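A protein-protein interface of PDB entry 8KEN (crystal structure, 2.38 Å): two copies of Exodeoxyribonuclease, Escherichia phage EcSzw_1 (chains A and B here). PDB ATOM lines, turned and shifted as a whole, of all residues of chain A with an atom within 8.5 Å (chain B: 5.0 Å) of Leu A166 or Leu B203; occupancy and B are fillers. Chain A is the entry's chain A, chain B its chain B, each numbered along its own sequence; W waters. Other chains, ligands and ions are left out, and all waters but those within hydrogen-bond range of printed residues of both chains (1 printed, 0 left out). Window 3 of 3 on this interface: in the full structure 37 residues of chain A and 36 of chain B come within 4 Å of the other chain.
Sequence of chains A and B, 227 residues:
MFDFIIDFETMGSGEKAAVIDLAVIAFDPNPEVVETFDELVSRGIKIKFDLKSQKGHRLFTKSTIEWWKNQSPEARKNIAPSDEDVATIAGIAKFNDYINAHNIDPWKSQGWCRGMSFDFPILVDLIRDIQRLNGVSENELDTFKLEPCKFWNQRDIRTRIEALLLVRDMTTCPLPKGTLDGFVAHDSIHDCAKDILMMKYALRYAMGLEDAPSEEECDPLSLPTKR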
ATOM      1  N   THR A 159     -29.933  -7.826  -6.541  1.00  0.00           N
ATOM      2  CA  THR A 159     -29.165  -7.659  -5.312  1.00  0.00           C
ATOM      3  C   THR A 159     -29.730  -8.512  -4.185  1.00  0.00           C
ATOM      4  O   THR A 159     -28.971  -9.121  -3.417  1.00  0.00           O
ATOM      5  CB  THR A 159     -29.143  -6.183  -4.923  1.00  0.00           C
ATOM      6  OG1 THR A 159     -28.667  -5.407  -6.037  1.00  0.00           O
ATOM      7  CG2 THR A 159     -28.269  -5.944  -3.724  1.00  0.00           C
ATOM      8  N   ARG A 160     -31.060  -8.582  -4.085  1.00  0.00           N
ATOM      9  CA  ARG A 160     -31.711  -9.405  -3.067  1.00  0.00           C
ATOM     10  C   ARG A 160     -31.299 -10.874  -3.180  1.00  0.00           C
ATOM     11  O   ARG A 160     -30.746 -11.455  -2.238  1.00  0.00           O
ATOM     12  CB  ARG A 160     -33.221  -9.271  -3.197  1.00  0.00           C
ATOM     13  CG  ARG A 160     -34.014 -10.137  -2.257  1.00  0.00           C
ATOM     14  CD  ARG A 160     -33.871  -9.698  -0.805  1.00  0.00           C
ATOM     15  NE  ARG A 160     -34.931 -10.280   0.009  1.00  0.00           N
ATOM     16  CZ  ARG A 160     -35.137 -10.016   1.293  1.00  0.00           C
ATOM     17  NH1 ARG A 160     -34.376  -9.160   1.952  1.00  0.00           N
ATOM     18  NH2 ARG A 160     -36.132 -10.631   1.933  1.00  0.00           N
ATOM     19  N   ILE A 161     -31.562 -11.490  -4.341  1.00  0.00           N
ATOM     20  CA  ILE A 161     -31.335 -12.925  -4.515  1.00  0.00           C
ATOM     21  C   ILE A 161     -29.856 -13.259  -4.365  1.00  0.00           C
ATOM     22  O   ILE A 161     -29.493 -14.224  -3.682  1.00  0.00           O
ATOM     23  CB  ILE A 161     -31.890 -13.394  -5.871  1.00  0.00           C
ATOM     24  CG1 ILE A 161     -33.405 -13.193  -5.932  1.00  0.00           C
ATOM     25  CG2 ILE A 161     -31.579 -14.855  -6.101  1.00  0.00           C
ATOM     26  CD1 ILE A 161     -34.003 -13.575  -7.265  1.00  0.00           C
ATOM     27  N   GLU A 162     -28.982 -12.470  -4.988  1.00  0.00           N
ATOM     28  CA  GLU A 162     -27.551 -12.717  -4.879  1.00  0.00           C
ATOM     29  C   GLU A 162     -27.089 -12.672  -3.431  1.00  0.00           C
ATOM     30  O   GLU A 162     -26.257 -13.486  -3.013  1.00  0.00           O
ATOM     31  CB  GLU A 162     -26.786 -11.690  -5.710  1.00  0.00           C
ATOM     32  CG  GLU A 162     -25.297 -11.833  -5.686  1.00  0.00           C
ATOM     33  CD  GLU A 162     -24.620 -10.630  -6.296  1.00  0.00           C
ATOM     34  OE1 GLU A 162     -24.802  -9.530  -5.738  1.00  0.00           O
ATOM     35  OE2 GLU A 162     -23.911 -10.768  -7.320  1.00  0.00           O
ATOM     36  N   ALA A 163     -27.619 -11.729  -2.651  1.00  0.00           N
ATOM     37  CA  ALA A 163     -27.237 -11.590  -1.253  1.00  0.00           C
ATOM     38  C   ALA A 163     -27.851 -12.676  -0.383  1.00  0.00           C
ATOM     39  O   ALA A 163     -27.242 -13.090   0.610  1.00  0.00           O
ATOM     40  CB  ALA A 163     -27.659 -10.221  -0.725  1.00  0.00           C
ATOM     41  N   LEU A 164     -29.062 -13.118  -0.712  1.00  0.00           N
ATOM     42  CA  LEU A 164     -29.694 -14.148   0.095  1.00  0.00           C
ATOM     43  C   LEU A 164     -28.940 -15.466  -0.029  1.00  0.00           C
ATOM     44  O   LEU A 164     -28.745 -16.167   0.971  1.00  0.00           O
ATOM     45  CB  LEU A 164     -31.160 -14.295  -0.306  1.00  0.00           C
ATOM     46  CG  LEU A 164     -32.077 -13.141   0.122  1.00  0.00           C
ATOM     47  CD1 LEU A 164     -33.527 -13.378  -0.293  1.00  0.00           C
ATOM     48  CD2 LEU A 164     -32.009 -12.913   1.620  1.00  0.00           C
ATOM     49  N   LEU A 165     -28.458 -15.789  -1.233  1.00  0.00           N
ATOM     50  CA  LEU A 165     -27.812 -17.070  -1.504  1.00  0.00           C
ATOM     51  C   LEU A 165     -26.296 -17.029  -1.344  1.00  0.00           C
ATOM     52  O   LEU A 165     -25.642 -18.074  -1.455  1.00  0.00           O
ATOM     53  CB  LEU A 165     -28.167 -17.532  -2.920  1.00  0.00           C
ATOM     54  CG  LEU A 165     -29.662 -17.439  -3.237  1.00  0.00           C
ATOM     55  CD1 LEU A 165     -29.915 -17.842  -4.664  1.00  0.00           C
ATOM     56  CD2 LEU A 165     -30.488 -18.285  -2.287  1.00  0.00           C
ATOM     57  N   LEU A 166     -25.725 -15.849  -1.103  1.00  0.00           N
ATOM     58  CA  LEU A 166     -24.288 -15.669  -0.886  1.00  0.00           C
ATOM     59  C   LEU A 166     -23.441 -16.219  -2.032  1.00  0.00           C
ATOM     60  O   LEU A 166     -22.329 -16.696  -1.804  1.00  0.00           O
ATOM     61  CB  LEU A 166     -23.844 -16.288   0.442  1.00  0.00           C
ATOM     62  CG  LEU A 166     -24.456 -15.680   1.705  1.00  0.00           C
ATOM     63  CD1 LEU A 166     -24.470 -16.677   2.845  1.00  0.00           C
ATOM     64  CD2 LEU A 166     -23.719 -14.421   2.101  1.00  0.00           C
ATOM     65  N   VAL A 167     -23.937 -16.143  -3.270  1.00  0.00           N
ATOM     66  CA  VAL A 167     -23.194 -16.550  -4.469  1.00  0.00           C
ATOM     67  C   VAL A 167     -23.155 -15.366  -5.431  1.00  0.00           C
ATOM     68  O   VAL A 167     -24.169 -15.044  -6.071  1.00  0.00           O
ATOM     69  CB  VAL A 167     -23.823 -17.775  -5.152  1.00  0.00           C
ATOM     70  CG1 VAL A 167     -22.935 -18.261  -6.298  1.00  0.00           C
ATOM     71  CG2 VAL A 167     -24.086 -18.891  -4.157  1.00  0.00           C
ATOM     72  N   ARG A 168     -21.984 -14.736  -5.557  1.00  0.00           N
ATOM     73  CA  ARG A 168     -21.822 -13.624  -6.487  1.00  0.00           C
ATOM     74  C   ARG A 168     -22.320 -14.006  -7.878  1.00  0.00           C
ATOM     75  O   ARG A 168     -22.087 -15.121  -8.353  1.00  0.00           O
ATOM     76  CB  ARG A 168     -20.350 -13.194  -6.564  1.00  0.00           C
ATOM     77  CG  ARG A 168     -20.057 -12.153  -7.651  1.00  0.00           C
ATOM     78  CD  ARG A 168     -18.830 -11.310  -7.302  1.00  0.00           C
ATOM     79  NE  ARG A 168     -18.546 -10.243  -8.262  1.00  0.00           N
ATOM     80  CZ  ARG A 168     -18.246  -8.997  -7.909  1.00  0.00           C
ATOM     81  NH1 ARG A 168     -18.185  -8.639  -6.631  1.00  0.00           N
ATOM     82  NH2 ARG A 168     -18.024  -8.079  -8.858  1.00  0.00           N
ATOM     83  N   ASP A 169     -23.036 -13.073  -8.513  1.00  0.00           N
ATOM     84  CA  ASP A 169     -23.504 -13.155  -9.894  1.00  0.00           C
ATOM     85  C   ASP A 169     -24.661 -14.120 -10.066  1.00  0.00           C
ATOM     86  O   ASP A 169     -25.052 -14.403 -11.205  1.00  0.00           O
ATOM     87  CB  ASP A 169     -22.376 -13.525 -10.871  1.00  0.00           C
ATOM     88  N   MET A 170     -25.242 -14.616  -8.972  1.00  0.00           N
ATOM     89  CA  MET A 170     -26.359 -15.556  -9.026  1.00  0.00           C
ATOM     90  C   MET A 170     -27.633 -14.778  -8.722  1.00  0.00           C
ATOM     91  O   MET A 170     -27.952 -14.503  -7.560  1.00  0.00           O
ATOM     92  CB  MET A 170     -26.156 -16.704  -8.045  1.00  0.00           C
ATOM     93  CG  MET A 170     -27.312 -17.699  -8.024  1.00  0.00           C
ATOM     94  SD  MET A 170     -26.789 -19.360  -7.528  1.00  0.00           S
ATOM     95  CE  MET A 170     -28.294 -20.010  -6.820  1.00  0.00           C
ATOM     96  N   ALA A 202     -35.574 -17.892  -2.008  1.00  0.00           N
ATOM     97  CA  ALA A 202     -34.274 -17.424  -1.537  1.00  0.00           C
ATOM     98  C   ALA A 202     -34.353 -16.964  -0.085  1.00  0.00           C
ATOM     99  O   ALA A 202     -33.429 -17.200   0.698  1.00  0.00           O
ATOM    100  CB  ALA A 202     -33.764 -16.296  -2.428  1.00  0.00           C
ATOM    101  N   ALA A 206     -32.238 -18.952   3.042  1.00  0.00           N
ATOM    102  CA  ALA A 206     -31.281 -18.204   3.853  1.00  0.00           C
ATOM    103  C   ALA A 206     -31.705 -18.139   5.313  1.00  0.00           C
ATOM    104  O   ALA A 206     -30.855 -17.979   6.194  1.00  0.00           O
ATOM    105  CB  ALA A 206     -31.092 -16.792   3.292  1.00  0.00           C
ATOM    106  N   PRO B  29     -14.074  -6.634  -3.205  1.00  0.00           N
ATOM    107  CA  PRO B  29     -15.279  -7.388  -2.812  1.00  0.00           C
ATOM    108  C   PRO B  29     -15.009  -8.551  -1.878  1.00  0.00           C
ATOM    109  O   PRO B  29     -15.957  -9.029  -1.240  1.00  0.00           O
ATOM    110  CB  PRO B  29     -15.825  -7.897  -4.152  1.00  0.00           C
ATOM    111  CG  PRO B  29     -14.597  -7.930  -5.055  1.00  0.00           C
ATOM    112  CD  PRO B  29     -13.798  -6.733  -4.648  1.00  0.00           C
ATOM    113  N   PRO B  31     -14.670 -11.123   0.901  1.00  0.00           N
ATOM    114  CA  PRO B  31     -15.053 -11.016   2.318  1.00  0.00           C
ATOM    115  C   PRO B  31     -13.863 -11.023   3.261  1.00  0.00           C
ATOM    116  O   PRO B  31     -13.819 -10.222   4.199  1.00  0.00           O
ATOM    117  CB  PRO B  31     -15.951 -12.247   2.537  1.00  0.00           C
ATOM    118  CG  PRO B  31     -16.346 -12.706   1.183  1.00  0.00           C
ATOM    119  CD  PRO B  31     -15.235 -12.318   0.254  1.00  0.00           C
ATOM    120  N   ARG B 160     -28.867  -4.804  -0.309  1.00  0.00           N
ATOM    121  CA  ARG B 160     -27.802  -5.705   0.137  1.00  0.00           C
ATOM    122  C   ARG B 160     -27.772  -5.828   1.656  1.00  0.00           C
ATOM    123  O   ARG B 160     -27.995  -6.908   2.212  1.00  0.00           O
ATOM    124  CB  ARG B 160     -26.456  -5.201  -0.378  1.00  0.00           C
ATOM    125  CG  ARG B 160     -25.244  -5.996   0.066  1.00  0.00           C
ATOM    126  CD  ARG B 160     -25.080  -7.254  -0.756  1.00  0.00           C
ATOM    127  NE  ARG B 160     -23.747  -7.816  -0.594  1.00  0.00           N
ATOM    128  CZ  ARG B 160     -23.387  -9.021  -1.008  1.00  0.00           C
ATOM    129  NH1 ARG B 160     -24.230  -9.804  -1.669  1.00  0.00           N
ATOM    130  NH2 ARG B 160     -22.153  -9.455  -0.748  1.00  0.00           N
ATOM    131  N   LEU B 164     -28.470  -9.188   3.878  1.00  0.00           N
ATOM    132  CA  LEU B 164     -27.439  -9.908   4.618  1.00  0.00           C
ATOM    133  C   LEU B 164     -27.797 -10.048   6.094  1.00  0.00           C
ATOM    134  O   LEU B 164     -27.505 -11.082   6.707  1.00  0.00           O
ATOM    135  CB  LEU B 164     -26.100  -9.193   4.449  1.00  0.00           C
ATOM    136  CG  LEU B 164     -25.596  -9.329   3.010  1.00  0.00           C
ATOM    137  CD1 LEU B 164     -24.371  -8.441   2.746  1.00  0.00           C
ATOM    138  CD2 LEU B 164     -25.290 -10.794   2.683  1.00  0.00           C
ATOM    139  N   MET B 199     -21.209  -2.610   4.259  1.00  0.00           N
ATOM    140  CA  MET B 199     -21.558  -3.727   3.391  1.00  0.00           C
ATOM    141  C   MET B 199     -20.655  -4.921   3.669  1.00  0.00           C
ATOM    142  O   MET B 199     -21.130  -6.060   3.746  1.00  0.00           O
ATOM    143  CB  MET B 199     -21.438  -3.294   1.931  1.00  0.00           C
ATOM    144  CG  MET B 199     -22.761  -2.868   1.291  1.00  0.00           C
ATOM    145  SD  MET B 199     -22.523  -2.554  -0.480  1.00  0.00           S
ATOM    146  CE  MET B 199     -21.112  -1.445  -0.474  1.00  0.00           C
ATOM    147  N   LYS B 200     -19.349  -4.672   3.827  1.00  0.00           N
ATOM    148  CA  LYS B 200     -18.399  -5.742   4.119  1.00  0.00           C
ATOM    149  C   LYS B 200     -18.768  -6.471   5.404  1.00  0.00           C
ATOM    150  O   LYS B 200     -18.939  -7.697   5.416  1.00  0.00           O
ATOM    151  CB  LYS B 200     -16.985  -5.169   4.219  1.00  0.00           C
ATOM    152  N   TYR B 201     -18.913  -5.727   6.500  1.00  0.00           N
ATOM    153  CA  TYR B 201     -19.164  -6.380   7.778  1.00  0.00           C
ATOM    154  C   TYR B 201     -20.490  -7.124   7.754  1.00  0.00           C
ATOM    155  O   TYR B 201     -20.571  -8.257   8.239  1.00  0.00           O
ATOM    156  CB  TYR B 201     -19.097  -5.362   8.920  1.00  0.00           C
ATOM    157  CG  TYR B 201     -17.661  -5.103   9.348  1.00  0.00           C
ATOM    158  CD1 TYR B 201     -16.911  -4.086   8.760  1.00  0.00           C
ATOM    159  CD2 TYR B 201     -17.035  -5.912  10.297  1.00  0.00           C
ATOM    160  CE1 TYR B 201     -15.601  -3.858   9.129  1.00  0.00           C
ATOM    161  CE2 TYR B 201     -15.719  -5.692  10.668  1.00  0.00           C
ATOM    162  CZ  TYR B 201     -15.014  -4.662  10.085  1.00  0.00           C
ATOM    163  OH  TYR B 201     -13.706  -4.435  10.446  1.00  0.00           O
ATOM    164  N   ALA B 202     -21.524  -6.532   7.144  1.00  0.00           N
ATOM    165  CA  ALA B 202     -22.789  -7.246   6.968  1.00  0.00           C
ATOM    166  C   ALA B 202     -22.583  -8.576   6.248  1.00  0.00           C
ATOM    167  O   ALA B 202     -23.214  -9.583   6.590  1.00  0.00           O
ATOM    168  CB  ALA B 202     -23.790  -6.373   6.205  1.00  0.00           C
ATOM    169  N   LEU B 203     -21.713  -8.599   5.240  1.00  0.00           N
ATOM    170  CA  LEU B 203     -21.374  -9.864   4.606  1.00  0.00           C
ATOM    171  C   LEU B 203     -20.697 -10.799   5.600  1.00  0.00           C
ATOM    172  O   LEU B 203     -21.023 -11.989   5.673  1.00  0.00           O
ATOM    173  CB  LEU B 203     -20.478  -9.624   3.392  1.00  0.00           C
ATOM    174  CG  LEU B 203     -20.132 -10.873   2.578  1.00  0.00           C
ATOM    175  CD1 LEU B 203     -21.367 -11.620   2.139  1.00  0.00           C
ATOM    176  CD2 LEU B 203     -19.251 -10.529   1.391  1.00  0.00           C
ATOM    177  N   ARG B 204     -19.767 -10.271   6.394  1.00  0.00           N
ATOM    178  CA  ARG B 204     -19.076 -11.115   7.361  1.00  0.00           C
ATOM    179  C   ARG B 204     -20.040 -11.647   8.418  1.00  0.00           C
ATOM    180  O   ARG B 204     -19.998 -12.833   8.762  1.00  0.00           O
ATOM    181  CB  ARG B 204     -17.922 -10.345   8.002  1.00  0.00           C
ATOM    182  N   TYR B 205     -20.940 -10.803   8.923  1.00  0.00           N
ATOM    183  CA  TYR B 205     -21.902 -11.293   9.907  1.00  0.00           C
ATOM    184  C   TYR B 205     -22.851 -12.322   9.311  1.00  0.00           C
ATOM    185  O   TYR B 205     -23.426 -13.124  10.057  1.00  0.00           O
ATOM    186  CB  TYR B 205     -22.723 -10.152  10.512  1.00  0.00           C
ATOM    187  CG  TYR B 205     -21.921  -8.981  11.033  1.00  0.00           C
ATOM    188  CD1 TYR B 205     -20.585  -9.128  11.418  1.00  0.00           C
ATOM    189  CD2 TYR B 205     -22.506  -7.724  11.163  1.00  0.00           C
ATOM    190  CE1 TYR B 205     -19.854  -8.047  11.893  1.00  0.00           C
ATOM    191  CE2 TYR B 205     -21.789  -6.644  11.644  1.00  0.00           C
ATOM    192  CZ  TYR B 205     -20.467  -6.806  12.003  1.00  0.00           C
ATOM    193  OH  TYR B 205     -19.755  -5.723  12.470  1.00  0.00           O
ATOM    194  N   ALA B 206     -23.038 -12.313   7.992  1.00  0.00           N
ATOM    195  CA  ALA B 206     -23.896 -13.303   7.358  1.00  0.00           C
ATOM    196  C   ALA B 206     -23.156 -14.606   7.110  1.00  0.00           C
ATOM    197  O   ALA B 206     -23.758 -15.683   7.195  1.00  0.00           O
ATOM    198  CB  ALA B 206     -24.443 -12.754   6.042  1.00  0.00           C
ATOM    199  N   MET B 207     -21.858 -14.520   6.806  1.00  0.00           N
ATOM    200  CA  MET B 207     -21.012 -15.680   6.553  1.00  0.00           C
ATOM    201  C   MET B 207     -20.427 -16.304   7.819  1.00  0.00           C
ATOM    202  O   MET B 207     -19.660 -17.268   7.708  1.00  0.00           O
ATOM    203  CB  MET B 207     -19.855 -15.298   5.626  1.00  0.00           C
ATOM    204  CG  MET B 207     -20.241 -14.969   4.200  1.00  0.00           C
ATOM    205  SD  MET B 207     -18.769 -14.688   3.206  1.00  0.00           S
ATOM    206  CE  MET B 207     -19.140 -15.677   1.758  1.00  0.00           C
HETATM  207  O   HOH W   1     -26.258  -8.594  -3.393  1.00  0.00           O
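Hydrophobic or aromatic side chains of chain A within 4 Å of the printed part of chain B: Ala A163 and Leu A166.
Of the 13 printed residues of chain B, 4 touch a printed residue of chain A.
Hydrophobic or aromatic side chains of chain B that line the printed part of chain A: Pro B29, Leu B164 and Leu B203.
Among the printed residues, 6 pairs touch across the chains.
Among the printed residues, merely in contact across the chains: Arg A168 with Pro B29, Ala A163 with Arg B160, Thr A159 with Arg B160, Leu A166 with Leu B203, Ala A163 with Leu B164 and Leu A166 with Leu B164.
Water W1 lies within hydrogen-bond range of O of Thr A159, OE1 of Glu A162, NH1 of Arg B160 and N of Ala A163.
Positions printed for both chains: 160, 164, 202 and 206.
Of the 6 pairs that touch across the chains among the printed residues, none has its exchanged pair printed and touching as well.
Of the printed residues of chain B, Leu A166 touches Leu B164 and Leu B203.
Val A167 touches none of the printed residues of chain B.
Of the printed residues of chain B, Arg A168 touches Pro B29 (3.5 Å).
Printed residues of chain A within 4 Å of Leu B164: Ala A163 (3.7 Å) and Leu A166 (3.995 Å).
No residue of chain A comes within 4 Å of Ala B202.
Printed residues of chain A within 4 Å of Leu B203: Leu A166 (3.7 Å).
No residue of chain A comes within 4 Å of Arg B204.
The nearest residue of chain A that does not touch Leu B203 is Ala A163 (6.2 Å).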
